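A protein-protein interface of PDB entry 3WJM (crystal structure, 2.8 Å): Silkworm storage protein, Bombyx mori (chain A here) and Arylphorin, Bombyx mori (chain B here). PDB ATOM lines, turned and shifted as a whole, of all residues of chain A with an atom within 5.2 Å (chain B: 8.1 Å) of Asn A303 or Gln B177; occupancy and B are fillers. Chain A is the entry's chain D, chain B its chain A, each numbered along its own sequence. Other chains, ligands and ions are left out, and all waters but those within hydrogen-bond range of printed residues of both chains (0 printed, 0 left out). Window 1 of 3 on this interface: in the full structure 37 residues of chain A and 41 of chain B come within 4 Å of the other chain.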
ATOM      1  N   MET A 170     -23.809  13.812 -23.148  1.00  0.00           N
ATOM      2  CA  MET A 170     -24.104  13.700 -21.719  1.00  0.00           C
ATOM      3  C   MET A 170     -24.814  12.420 -21.296  1.00  0.00           C
ATOM      4  O   MET A 170     -24.458  11.833 -20.283  1.00  0.00           O
ATOM      5  CB  MET A 170     -24.988  14.838 -21.292  1.00  0.00           C
ATOM      6  CG  MET A 170     -24.296  15.884 -20.472  1.00  0.00           C
ATOM      7  SD  MET A 170     -25.627  16.888 -19.796  1.00  0.00           S
ATOM      8  CE  MET A 170     -26.044  15.998 -18.287  1.00  0.00           C
ATOM      9  N   LYS A 173     -22.327   9.557 -21.036  1.00  0.00           N
ATOM     10  CA  LYS A 173     -21.380   9.902 -19.981  1.00  0.00           C
ATOM     11  C   LYS A 173     -21.989   9.703 -18.602  1.00  0.00           C
ATOM     12  O   LYS A 173     -21.330   9.192 -17.688  1.00  0.00           O
ATOM     13  CB  LYS A 173     -20.959  11.363 -20.118  1.00  0.00           C
ATOM     14  CG  LYS A 173     -19.545  11.661 -19.684  1.00  0.00           C
ATOM     15  CD  LYS A 173     -19.452  12.802 -18.681  1.00  0.00           C
ATOM     16  CE  LYS A 173     -18.383  12.463 -17.634  1.00  0.00           C
ATOM     17  NZ  LYS A 173     -18.480  13.182 -16.326  1.00  0.00           N
ATOM     18  N   PRO A 301     -24.590  19.095 -26.065  1.00  0.00           N
ATOM     19  CA  PRO A 301     -24.899  18.201 -24.920  1.00  0.00           C
ATOM     20  C   PRO A 301     -23.612  17.887 -24.128  1.00  0.00           C
ATOM     21  O   PRO A 301     -23.186  16.723 -24.006  1.00  0.00           O
ATOM     22  CB  PRO A 301     -25.496  16.961 -25.600  1.00  0.00           C
ATOM     23  CG  PRO A 301     -24.893  16.957 -26.979  1.00  0.00           C
ATOM     24  CD  PRO A 301     -24.287  18.313 -27.279  1.00  0.00           C
ATOM     25  N   PHE A 302     -22.997  18.952 -23.621  1.00  0.00           N
ATOM     26  CA  PHE A 302     -21.741  18.860 -22.923  1.00  0.00           C
ATOM     27  C   PHE A 302     -21.728  19.776 -21.723  1.00  0.00           C
ATOM     28  O   PHE A 302     -22.459  20.780 -21.693  1.00  0.00           O
ATOM     29  CB  PHE A 302     -20.598  19.270 -23.832  1.00  0.00           C
ATOM     30  CG  PHE A 302     -20.443  18.421 -25.048  1.00  0.00           C
ATOM     31  CD1 PHE A 302     -20.535  18.988 -26.306  1.00  0.00           C
ATOM     32  CD2 PHE A 302     -20.142  17.072 -24.942  1.00  0.00           C
ATOM     33  CE1 PHE A 302     -20.330  18.224 -27.444  1.00  0.00           C
ATOM     34  CE2 PHE A 302     -19.926  16.295 -26.060  1.00  0.00           C
ATOM     35  CZ  PHE A 302     -20.024  16.872 -27.318  1.00  0.00           C
ATOM     36  N   ASN A 303     -20.892  19.408 -20.742  1.00  0.00           N
ATOM     37  CA  ASN A 303     -20.533  20.291 -19.625  1.00  0.00           C
ATOM     38  C   ASN A 303     -19.075  20.203 -19.188  1.00  0.00           C
ATOM     39  O   ASN A 303     -18.417  19.226 -19.416  1.00  0.00           O
ATOM     40  CB  ASN A 303     -21.437  20.062 -18.431  1.00  0.00           C
ATOM     41  CG  ASN A 303     -21.622  18.612 -18.121  1.00  0.00           C
ATOM     42  OD1 ASN A 303     -22.327  17.923 -18.832  1.00  0.00           O
ATOM     43  ND2 ASN A 303     -21.012  18.141 -17.044  1.00  0.00           N
ATOM     44  N   SER A 304     -18.578  21.265 -18.589  1.00  0.00           N
ATOM     45  CA  SER A 304     -17.223  21.341 -18.107  1.00  0.00           C
ATOM     46  C   SER A 304     -17.331  21.257 -16.595  1.00  0.00           C
ATOM     47  O   SER A 304     -18.401  21.124 -16.084  1.00  0.00           O
ATOM     48  CB  SER A 304     -16.646  22.681 -18.518  1.00  0.00           C
ATOM     49  OG  SER A 304     -17.221  23.700 -17.718  1.00  0.00           O
ATOM     50  N   PHE A 305     -16.233  21.343 -15.869  1.00  0.00           N
ATOM     51  CA  PHE A 305     -16.292  21.286 -14.410  1.00  0.00           C
ATOM     52  C   PHE A 305     -17.382  22.207 -13.783  1.00  0.00           C
ATOM     53  O   PHE A 305     -18.069  21.796 -12.843  1.00  0.00           O
ATOM     54  CB  PHE A 305     -14.877  21.588 -13.854  1.00  0.00           C
ATOM     55  CG  PHE A 305     -14.710  21.366 -12.368  1.00  0.00           C
ATOM     56  CD1 PHE A 305     -15.667  20.687 -11.613  1.00  0.00           C
ATOM     57  CD2 PHE A 305     -13.551  21.806 -11.743  1.00  0.00           C
ATOM     58  CE1 PHE A 305     -15.484  20.490 -10.250  1.00  0.00           C
ATOM     59  CE2 PHE A 305     -13.340  21.596 -10.387  1.00  0.00           C
ATOM     60  CZ  PHE A 305     -14.305  20.937  -9.633  1.00  0.00           C
ATOM     61  N   TYR A 306     -17.530  23.431 -14.295  1.00  0.00           N
ATOM     62  CA  TYR A 306     -18.433  24.434 -13.700  1.00  0.00           C
ATOM     63  C   TYR A 306     -19.717  24.737 -14.486  1.00  0.00           C
ATOM     64  O   TYR A 306     -20.689  25.177 -13.903  1.00  0.00           O
ATOM     65  CB  TYR A 306     -17.744  25.791 -13.565  1.00  0.00           C
ATOM     66  CG  TYR A 306     -16.531  25.866 -12.707  1.00  0.00           C
ATOM     67  CD1 TYR A 306     -16.256  24.898 -11.720  1.00  0.00           C
ATOM     68  CD2 TYR A 306     -15.652  26.940 -12.843  1.00  0.00           C
ATOM     69  CE1 TYR A 306     -15.119  24.987 -10.924  1.00  0.00           C
ATOM     70  CE2 TYR A 306     -14.531  27.045 -12.040  1.00  0.00           C
ATOM     71  CZ  TYR A 306     -14.276  26.079 -11.083  1.00  0.00           C
ATOM     72  OH  TYR A 306     -13.160  26.216 -10.300  1.00  0.00           O
ATOM     73  N   TYR A 307     -19.685  24.588 -15.803  1.00  0.00           N
ATOM     74  CA  TYR A 307     -20.712  25.153 -16.648  1.00  0.00           C
ATOM     75  C   TYR A 307     -21.227  24.119 -17.603  1.00  0.00           C
ATOM     76  O   TYR A 307     -20.456  23.369 -18.173  1.00  0.00           O
ATOM     77  CB  TYR A 307     -20.157  26.289 -17.505  1.00  0.00           C
ATOM     78  CG  TYR A 307     -19.351  27.350 -16.780  1.00  0.00           C
ATOM     79  CD1 TYR A 307     -17.957  27.435 -16.942  1.00  0.00           C
ATOM     80  CD2 TYR A 307     -19.981  28.308 -15.985  1.00  0.00           C
ATOM     81  CE1 TYR A 307     -17.209  28.431 -16.298  1.00  0.00           C
ATOM     82  CE2 TYR A 307     -19.246  29.304 -15.348  1.00  0.00           C
ATOM     83  CZ  TYR A 307     -17.869  29.363 -15.497  1.00  0.00           C
ATOM     84  OH  TYR A 307     -17.163  30.347 -14.829  1.00  0.00           O
ATOM     85  N   PRO A 308     -22.551  24.079 -17.777  1.00  0.00           N
ATOM     86  CA  PRO A 308     -23.082  23.506 -19.007  1.00  0.00           C
ATOM     87  C   PRO A 308     -22.588  24.352 -20.181  1.00  0.00           C
ATOM     88  O   PRO A 308     -22.504  25.550 -20.058  1.00  0.00           O
ATOM     89  CB  PRO A 308     -24.589  23.678 -18.844  1.00  0.00           C
ATOM     90  CG  PRO A 308     -24.744  24.792 -17.877  1.00  0.00           C
ATOM     91  CD  PRO A 308     -23.607  24.662 -16.924  1.00  0.00           C
ATOM     92  N   PHE A 309     -22.210  23.721 -21.286  1.00  0.00           N
ATOM     93  CA  PHE A 309     -21.863  24.449 -22.503  1.00  0.00           C
ATOM     94  C   PHE A 309     -22.953  25.456 -22.869  1.00  0.00           C
ATOM     95  O   PHE A 309     -24.151  25.190 -22.671  1.00  0.00           O
ATOM     96  CB  PHE A 309     -21.642  23.479 -23.672  1.00  0.00           C
ATOM     97  CG  PHE A 309     -20.238  22.914 -23.763  1.00  0.00           C
ATOM     98  CD1 PHE A 309     -19.500  22.601 -22.618  1.00  0.00           C
ATOM     99  CD2 PHE A 309     -19.674  22.645 -24.997  1.00  0.00           C
ATOM    100  CE1 PHE A 309     -18.214  22.044 -22.709  1.00  0.00           C
ATOM    101  CE2 PHE A 309     -18.410  22.094 -25.102  1.00  0.00           C
ATOM    102  CZ  PHE A 309     -17.666  21.801 -23.960  1.00  0.00           C
ATOM    103  N   MET B 171     -28.644  22.712  -6.060  1.00  0.00           N
ATOM    104  CA  MET B 171     -27.176  22.842  -6.138  1.00  0.00           C
ATOM    105  C   MET B 171     -26.639  22.887  -7.561  1.00  0.00           C
ATOM    106  O   MET B 171     -27.128  22.183  -8.464  1.00  0.00           O
ATOM    107  CB  MET B 171     -26.498  21.708  -5.369  1.00  0.00           C
ATOM    108  CG  MET B 171     -26.796  20.303  -5.865  1.00  0.00           C
ATOM    109  SD  MET B 171     -25.833  19.042  -4.976  1.00  0.00           S
ATOM    110  CE  MET B 171     -27.027  18.009  -4.139  1.00  0.00           C
ATOM    111  N   ASN B 172     -25.621  23.702  -7.771  1.00  0.00           N
ATOM    112  CA  ASN B 172     -24.961  23.750  -9.081  1.00  0.00           C
ATOM    113  C   ASN B 172     -24.120  22.505  -9.377  1.00  0.00           C
ATOM    114  O   ASN B 172     -23.904  21.651  -8.517  1.00  0.00           O
ATOM    115  CB  ASN B 172     -24.145  25.026  -9.213  1.00  0.00           C
ATOM    116  CG  ASN B 172     -24.858  26.224  -8.614  1.00  0.00           C
ATOM    117  OD1 ASN B 172     -26.051  26.408  -8.797  1.00  0.00           O
ATOM    118  ND2 ASN B 172     -24.130  27.018  -7.844  1.00  0.00           N
ATOM    119  N   MET B 173     -23.683  22.403 -10.614  1.00  0.00           N
ATOM    120  CA  MET B 173     -23.073  21.197 -11.099  1.00  0.00           C
ATOM    121  C   MET B 173     -21.638  21.023 -10.602  1.00  0.00           C
ATOM    122  O   MET B 173     -21.137  19.904 -10.544  1.00  0.00           O
ATOM    123  CB  MET B 173     -23.123  21.156 -12.627  1.00  0.00           C
ATOM    124  CG  MET B 173     -22.486  22.356 -13.303  1.00  0.00           C
ATOM    125  SD  MET B 173     -22.135  22.153 -15.059  1.00  0.00           S
ATOM    126  CE  MET B 173     -23.692  21.644 -15.754  1.00  0.00           C
ATOM    127  N   GLU B 174     -20.973  22.107 -10.247  1.00  0.00           N
ATOM    128  CA  GLU B 174     -19.663  21.991  -9.660  1.00  0.00           C
ATOM    129  C   GLU B 174     -19.666  21.027  -8.449  1.00  0.00           C
ATOM    130  O   GLU B 174     -18.947  20.020  -8.433  1.00  0.00           O
ATOM    131  CB  GLU B 174     -19.193  23.349  -9.225  1.00  0.00           C
ATOM    132  CG  GLU B 174     -17.824  23.337  -8.621  1.00  0.00           C
ATOM    133  CD  GLU B 174     -17.385  24.739  -8.320  1.00  0.00           C
ATOM    134  OE1 GLU B 174     -18.186  25.657  -8.642  1.00  0.00           O
ATOM    135  OE2 GLU B 174     -16.259  24.925  -7.783  1.00  0.00           O
ATOM    136  N   VAL B 175     -20.477  21.344  -7.439  1.00  0.00           N
ATOM    137  CA  VAL B 175     -20.596  20.506  -6.251  1.00  0.00           C
ATOM    138  C   VAL B 175     -21.042  19.118  -6.632  1.00  0.00           C
ATOM    139  O   VAL B 175     -20.619  18.107  -6.033  1.00  0.00           O
ATOM    140  CB  VAL B 175     -21.667  21.020  -5.295  1.00  0.00           C
ATOM    141  CG1 VAL B 175     -21.361  20.506  -3.901  1.00  0.00           C
ATOM    142  CG2 VAL B 175     -21.722  22.537  -5.327  1.00  0.00           C
ATOM    143  N   LEU B 176     -21.911  19.070  -7.629  1.00  0.00           N
ATOM    144  CA  LEU B 176     -22.482  17.814  -8.009  1.00  0.00           C
ATOM    145  C   LEU B 176     -21.370  16.933  -8.533  1.00  0.00           C
ATOM    146  O   LEU B 176     -21.312  15.752  -8.216  1.00  0.00           O
ATOM    147  CB  LEU B 176     -23.555  18.014  -9.060  1.00  0.00           C
ATOM    148  CG  LEU B 176     -24.408  16.787  -9.365  1.00  0.00           C
ATOM    149  CD1 LEU B 176     -24.869  16.105  -8.076  1.00  0.00           C
ATOM    150  CD2 LEU B 176     -25.569  17.182 -10.290  1.00  0.00           C
ATOM    151  N   GLN B 177     -20.462  17.518  -9.297  1.00  0.00           N
ATOM    152  CA  GLN B 177     -19.439  16.714  -9.935  1.00  0.00           C
ATOM    153  C   GLN B 177     -18.368  16.255  -8.998  1.00  0.00           C
ATOM    154  O   GLN B 177     -17.839  15.152  -9.153  1.00  0.00           O
ATOM    155  CB  GLN B 177     -18.906  17.368 -11.201  1.00  0.00           C
ATOM    156  CG  GLN B 177     -20.053  17.419 -12.189  1.00  0.00           C
ATOM    157  CD  GLN B 177     -19.646  17.817 -13.579  1.00  0.00           C
ATOM    158  OE1 GLN B 177     -19.741  16.998 -14.508  1.00  0.00           O
ATOM    159  NE2 GLN B 177     -19.222  19.080 -13.748  1.00  0.00           N
ATOM    160  N   LYS B 178     -18.097  17.065  -7.990  1.00  0.00           N
ATOM    161  CA  LYS B 178     -17.200  16.648  -6.949  1.00  0.00           C
ATOM    162  C   LYS B 178     -17.800  15.447  -6.220  1.00  0.00           C
ATOM    163  O   LYS B 178     -17.106  14.453  -5.991  1.00  0.00           O
ATOM    164  CB  LYS B 178     -16.928  17.772  -5.975  1.00  0.00           C
ATOM    165  CG  LYS B 178     -16.183  18.905  -6.574  1.00  0.00           C
ATOM    166  CD  LYS B 178     -15.947  19.996  -5.562  1.00  0.00           C
ATOM    167  CE  LYS B 178     -15.685  21.279  -6.319  1.00  0.00           C
ATOM    168  NZ  LYS B 178     -15.052  22.296  -5.459  1.00  0.00           N
ATOM    169  N   ILE B 179     -19.087  15.537  -5.870  1.00  0.00           N
ATOM    170  CA  ILE B 179     -19.779  14.435  -5.210  1.00  0.00           C
ATOM    171  C   ILE B 179     -19.648  13.202  -6.086  1.00  0.00           C
ATOM    172  O   ILE B 179     -19.288  12.146  -5.598  1.00  0.00           O
ATOM    173  CB  ILE B 179     -21.251  14.797  -4.939  1.00  0.00           C
ATOM    174  CG1 ILE B 179     -21.342  15.787  -3.765  1.00  0.00           C
ATOM    175  CG2 ILE B 179     -22.112  13.572  -4.697  1.00  0.00           C
ATOM    176  CD1 ILE B 179     -22.648  16.583  -3.731  1.00  0.00           C
ATOM    177  N   TYR B 180     -19.881  13.345  -7.382  1.00  0.00           N
ATOM    178  CA  TYR B 180     -19.797  12.201  -8.290  1.00  0.00           C
ATOM    179  C   TYR B 180     -18.417  11.601  -8.343  1.00  0.00           C
ATOM    180  O   TYR B 180     -18.289  10.373  -8.252  1.00  0.00           O
ATOM    181  CB  TYR B 180     -20.218  12.551  -9.716  1.00  0.00           C
ATOM    182  CG  TYR B 180     -21.705  12.714  -9.918  1.00  0.00           C
ATOM    183  CD1 TYR B 180     -22.603  12.394  -8.920  1.00  0.00           C
ATOM    184  CD2 TYR B 180     -22.214  13.159 -11.133  1.00  0.00           C
ATOM    185  CE1 TYR B 180     -23.966  12.539  -9.105  1.00  0.00           C
ATOM    186  CE2 TYR B 180     -23.575  13.308 -11.327  1.00  0.00           C
ATOM    187  CZ  TYR B 180     -24.449  12.995 -10.306  1.00  0.00           C
ATOM    188  OH  TYR B 180     -25.817  13.128 -10.480  1.00  0.00           O
ATOM    189  N   VAL B 181     -17.399  12.458  -8.511  1.00  0.00           N
ATOM    190  CA  VAL B 181     -15.986  12.011  -8.632  1.00  0.00           C
ATOM    191  C   VAL B 181     -15.611  11.210  -7.369  1.00  0.00           C
ATOM    192  O   VAL B 181     -15.133  10.087  -7.456  1.00  0.00           O
ATOM    193  CB  VAL B 181     -14.990  13.202  -8.870  1.00  0.00           C
ATOM    194  CG1 VAL B 181     -13.550  12.748  -8.682  1.00  0.00           C
ATOM    195  CG2 VAL B 181     -15.191  13.874 -10.240  1.00  0.00           C
ATOM    196  N   THR B 182     -15.868  11.775  -6.192  1.00  0.00           N
ATOM    197  CA  THR B 182     -15.606  11.076  -4.930  1.00  0.00           C
ATOM    198  C   THR B 182     -16.281   9.689  -4.847  1.00  0.00           C
ATOM    199  O   THR B 182     -15.703   8.732  -4.356  1.00  0.00           O
ATOM    200  CB  THR B 182     -16.102  11.916  -3.753  1.00  0.00           C
ATOM    201  OG1 THR B 182     -15.409  13.150  -3.749  1.00  0.00           O
ATOM    202  CG2 THR B 182     -15.838  11.218  -2.444  1.00  0.00           C
ATOM    203  N   LYS B 183     -17.523   9.614  -5.309  1.00  0.00           N
ATOM    204  CA  LYS B 183     -18.242   8.367  -5.265  1.00  0.00           C
ATOM    205  C   LYS B 183     -17.601   7.344  -6.229  1.00  0.00           C
ATOM    206  O   LYS B 183     -17.327   6.187  -5.845  1.00  0.00           O
ATOM    207  CB  LYS B 183     -19.726   8.622  -5.548  1.00  0.00           C
ATOM    208  CG  LYS B 183     -20.621   7.429  -5.379  1.00  0.00           C
ATOM    209  CD  LYS B 183     -20.678   6.952  -3.939  1.00  0.00           C
ATOM    210  CE  LYS B 183     -21.556   5.692  -3.782  1.00  0.00           C
ATOM    211  NZ  LYS B 183     -20.927   4.448  -4.319  1.00  0.00           N
ATOM    212  N   MET B 184     -17.330   7.782  -7.458  1.00  0.00           N
ATOM    213  CA  MET B 184     -16.598   6.949  -8.411  1.00  0.00           C
ATOM    214  C   MET B 184     -15.239   6.456  -7.896  1.00  0.00           C
ATOM    215  O   MET B 184     -14.823   5.362  -8.237  1.00  0.00           O
ATOM    216  CB  MET B 184     -16.426   7.678  -9.737  1.00  0.00           C
ATOM    217  CG  MET B 184     -17.713   7.783 -10.538  1.00  0.00           C
ATOM    218  SD  MET B 184     -17.426   8.400 -12.214  1.00  0.00           S
ATOM    219  CE  MET B 184     -17.449  10.174 -11.926  1.00  0.00           C
ATOM    220  N   ILE B 199     -13.538  19.802   0.098  1.00  0.00           N
ATOM    221  CA  ILE B 199     -14.031  18.474   0.375  1.00  0.00           C
ATOM    222  C   ILE B 199     -13.284  17.897   1.544  1.00  0.00           C
ATOM    223  O   ILE B 199     -12.083  17.840   1.509  1.00  0.00           O
ATOM    224  CB  ILE B 199     -13.833  17.548  -0.828  1.00  0.00           C
ATOM    225  CG1 ILE B 199     -14.359  18.211  -2.114  1.00  0.00           C
ATOM    226  CG2 ILE B 199     -14.495  16.204  -0.554  1.00  0.00           C
ATOM    227  CD1 ILE B 199     -14.195  17.396  -3.381  1.00  0.00           C
ATOM    228  N   TYR B 208     -19.062  18.737   1.595  1.00  0.00           N
ATOM    229  CA  TYR B 208     -18.752  19.568   0.450  1.00  0.00           C
ATOM    230  C   TYR B 208     -19.246  20.977   0.607  1.00  0.00           C
ATOM    231  O   TYR B 208     -20.469  21.239   0.607  1.00  0.00           O
ATOM    232  CB  TYR B 208     -19.416  19.026  -0.809  1.00  0.00           C
ATOM    233  CG  TYR B 208     -18.963  17.667  -1.178  1.00  0.00           C
ATOM    234  CD1 TYR B 208     -17.927  17.488  -2.093  1.00  0.00           C
ATOM    235  CD2 TYR B 208     -19.580  16.553  -0.621  1.00  0.00           C
ATOM    236  CE1 TYR B 208     -17.511  16.219  -2.437  1.00  0.00           C
ATOM    237  CE2 TYR B 208     -19.155  15.286  -0.923  1.00  0.00           C
ATOM    238  CZ  TYR B 208     -18.124  15.118  -1.827  1.00  0.00           C
ATOM    239  OH  TYR B 208     -17.726  13.848  -2.112  1.00  0.00           O
ATOM    240  N   LEU B 304     -26.869  26.537 -13.918  1.00  0.00           N
ATOM    241  CA  LEU B 304     -25.764  25.584 -13.751  1.00  0.00           C
ATOM    242  C   LEU B 304     -26.240  24.273 -13.114  1.00  0.00           C
ATOM    243  O   LEU B 304     -25.448  23.567 -12.535  1.00  0.00           O
ATOM    244  CB  LEU B 304     -24.620  26.180 -12.912  1.00  0.00           C
ATOM    245  CG  LEU B 304     -24.164  27.620 -13.152  1.00  0.00           C
ATOM    246  CD1 LEU B 304     -23.235  28.090 -12.055  1.00  0.00           C
ATOM    247  CD2 LEU B 304     -23.514  27.801 -14.498  1.00  0.00           C
ATOM    248  N   MET B 305     -27.527  23.964 -13.198  1.00  0.00           N
ATOM    249  CA  MET B 305     -28.017  22.680 -12.731  1.00  0.00           C
ATOM    250  C   MET B 305     -28.033  21.627 -13.837  1.00  0.00           C
ATOM    251  O   MET B 305     -28.202  21.931 -15.037  1.00  0.00           O
ATOM    252  CB  MET B 305     -29.432  22.756 -12.139  1.00  0.00           C
ATOM    253  CG  MET B 305     -29.626  23.583 -10.886  1.00  0.00           C
ATOM    254  SD  MET B 305     -30.336  25.165 -11.360  1.00  0.00           S
ATOM    255  CE  MET B 305     -31.937  24.702 -12.014  1.00  0.00           C
ATOM    256  N   LEU B 306     -27.907  20.380 -13.385  1.00  0.00           N
ATOM    257  CA  LEU B 306     -27.954  19.197 -14.208  1.00  0.00           C
ATOM    258  C   LEU B 306     -29.097  18.295 -13.805  1.00  0.00           C
ATOM    259  O   LEU B 306     -29.435  18.169 -12.643  1.00  0.00           O
ATOM    260  CB  LEU B 306     -26.700  18.377 -13.964  1.00  0.00           C
ATOM    261  CG  LEU B 306     -25.363  18.793 -14.542  1.00  0.00           C
ATOM    262  CD1 LEU B 306     -24.335  17.778 -14.055  1.00  0.00           C
ATOM    263  CD2 LEU B 306     -25.431  18.870 -16.066  1.00  0.00           C
ATOM    264  N   PHE B 309     -29.881  13.497 -17.636  1.00  0.00           N
ATOM    265  CA  PHE B 309     -29.512  13.356 -19.059  1.00  0.00           C
ATOM    266  C   PHE B 309     -29.500  14.651 -19.899  1.00  0.00           C
ATOM    267  O   PHE B 309     -29.549  14.576 -21.132  1.00  0.00           O
ATOM    268  CB  PHE B 309     -30.413  12.300 -19.732  1.00  0.00           C
ATOM    269  CG  PHE B 309     -30.436  10.975 -19.016  1.00  0.00           C
ATOM    270  CD1 PHE B 309     -31.603  10.518 -18.406  1.00  0.00           C
ATOM    271  CD2 PHE B 309     -29.276  10.177 -18.934  1.00  0.00           C
ATOM    272  CE1 PHE B 309     -31.614   9.292 -17.739  1.00  0.00           C
ATOM    273  CE2 PHE B 309     -29.281   8.955 -18.264  1.00  0.00           C
ATOM    274  CZ  PHE B 309     -30.454   8.513 -17.666  1.00  0.00           C
ATOM    275  N   THR B 310     -29.455  15.813 -19.234  1.00  0.00           N
ATOM    276  CA  THR B 310     -29.476  17.153 -19.877  1.00  0.00           C
ATOM    277  C   THR B 310     -29.128  18.276 -18.907  1.00  0.00           C
ATOM    278  O   THR B 310     -29.369  18.150 -17.701  1.00  0.00           O
ATOM    279  CB  THR B 310     -30.875  17.570 -20.390  1.00  0.00           C
ATOM    280  OG1 THR B 310     -31.903  16.777 -19.770  1.00  0.00           O
ATOM    281  CG2 THR B 310     -30.964  17.538 -21.927  1.00  0.00           C
ATOM    282  N   PRO B 311     -28.609  19.402 -19.433  1.00  0.00           N
ATOM    283  CA  PRO B 311     -28.674  20.614 -18.617  1.00  0.00           C
ATOM    284  C   PRO B 311     -30.044  21.286 -18.763  1.00  0.00           C
ATOM    285  O   PRO B 311     -30.786  20.967 -19.699  1.00  0.00           O
ATOM    286  CB  PRO B 311     -27.578  21.490 -19.218  1.00  0.00           C
ATOM    287  CG  PRO B 311     -27.528  21.098 -20.658  1.00  0.00           C
ATOM    288  CD  PRO B 311     -27.957  19.647 -20.737  1.00  0.00           C
ATOM    289  N   SER B 482     -28.505  12.292  -4.286  1.00  0.00           N
ATOM    290  CA  SER B 482     -27.940  12.731  -5.561  1.00  0.00           C
ATOM    291  C   SER B 482     -27.020  11.669  -6.121  1.00  0.00           C
ATOM    292  O   SER B 482     -26.689  11.687  -7.314  1.00  0.00           O
ATOM    293  CB  SER B 482     -27.124  14.009  -5.379  1.00  0.00           C
ATOM    294  OG  SER B 482     -25.867  13.689  -4.866  1.00  0.00           O
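Of the printed residues of chain B, Asn A303 touches Met B173 and Gln B177.
Of chain A, only Asn A303, Ser A304 and Phe A305 come within 4 Å of Gln B177.
Of the printed residues of chain A, Leu B306 touches Met A170.
Printed residues of chain A within 4 Å of Glu B174: Phe A305 and Tyr A306.
Printed residues of chain B within 4 Å of Tyr A307: Met B173 and Leu B304.
Of the printed residues of chain A, Lys B178 touches Phe A305.
Of the printed residues of chain A, Pro B311 touches Met A170 (3.7 Å) and Pro A308 (3.7 Å).
Asn B172 touches none of the printed residues of chain A.
The nearest printed residue of chain B that does not touch Tyr A307 is Gln B177 (5.9 Å).
The backbone NH (N) of Met B173 lies within hydrogen-bond range of the backbone carbonyl oxygen (O) of Leu B304, 2.9 Å away.
O of Lys B178 lies within hydrogen-bond range of OG1 of Thr B182 (3.1 Å).
The backbone NH of Met A170 lies within hydrogen-bond range of the backbone carbonyl oxygen of Pro A301 (3.1 Å).
The side-chain sulfur (SD) of Met A170 sits close to the side-chain amide oxygen (OD1) of Asn A303, 3.6 Å away.
The side-chain hydroxyl of Ser A304 sits close to the backbone NH of Tyr A306 (3.4 Å).
The side-chain hydroxyl (OG) of Ser A304 lies within hydrogen-bond range of the backbone NH (N) of Tyr A307, 3.2 Å away.
Met A170 touches Leu B306.
Thr B310 touches Met A170 (N to CE, 3.5 Å).
Met A170 touches Pro B311.
CE of Met B173 touches CB of Asn A303, 3.8 Å away.
Phe A305 touches Glu B174.
Lys B178 touches Phe A305 (CE to CZ, 3.6 Å).
Glu B174 touches Tyr A306.
Tyr A306 touches Leu B304.
CD of Pro A308 touches CA of Leu B304, at 3.9 Å.
CB of Pro B311 touches CB of Pro A308, at 3.7 Å.
Of the 23 printed residues of chain B, 8 touch a printed residue of chain A.
Among the printed residues, 17 pairs touch across the chains.
Among the printed residues, no Asp or Glu carboxylate lies within 4 Å of a Lys or Arg side-chain nitrogen of the other chain.
SD of Met B173 lies close to N of Tyr A307.
OE1 of Gln B177 sits at hydrogen-bond distance from ND2 of Asn A303.
The backbone carbonyl oxygen (O) of Ser A304 sits at hydrogen-bond distance from the side-chain amide nitrogen (NE2) of Gln B177.
O of Phe A305 sits at hydrogen-bond distance from NE2 of Gln B177.
The backbone carbonyl oxygen (O) of Tyr A306 lies close to the side-chain sulfur (SD) of Met B173 (3.5 Å).
N of Pro A308 sits close to SD of Met B173 (3.4 Å).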
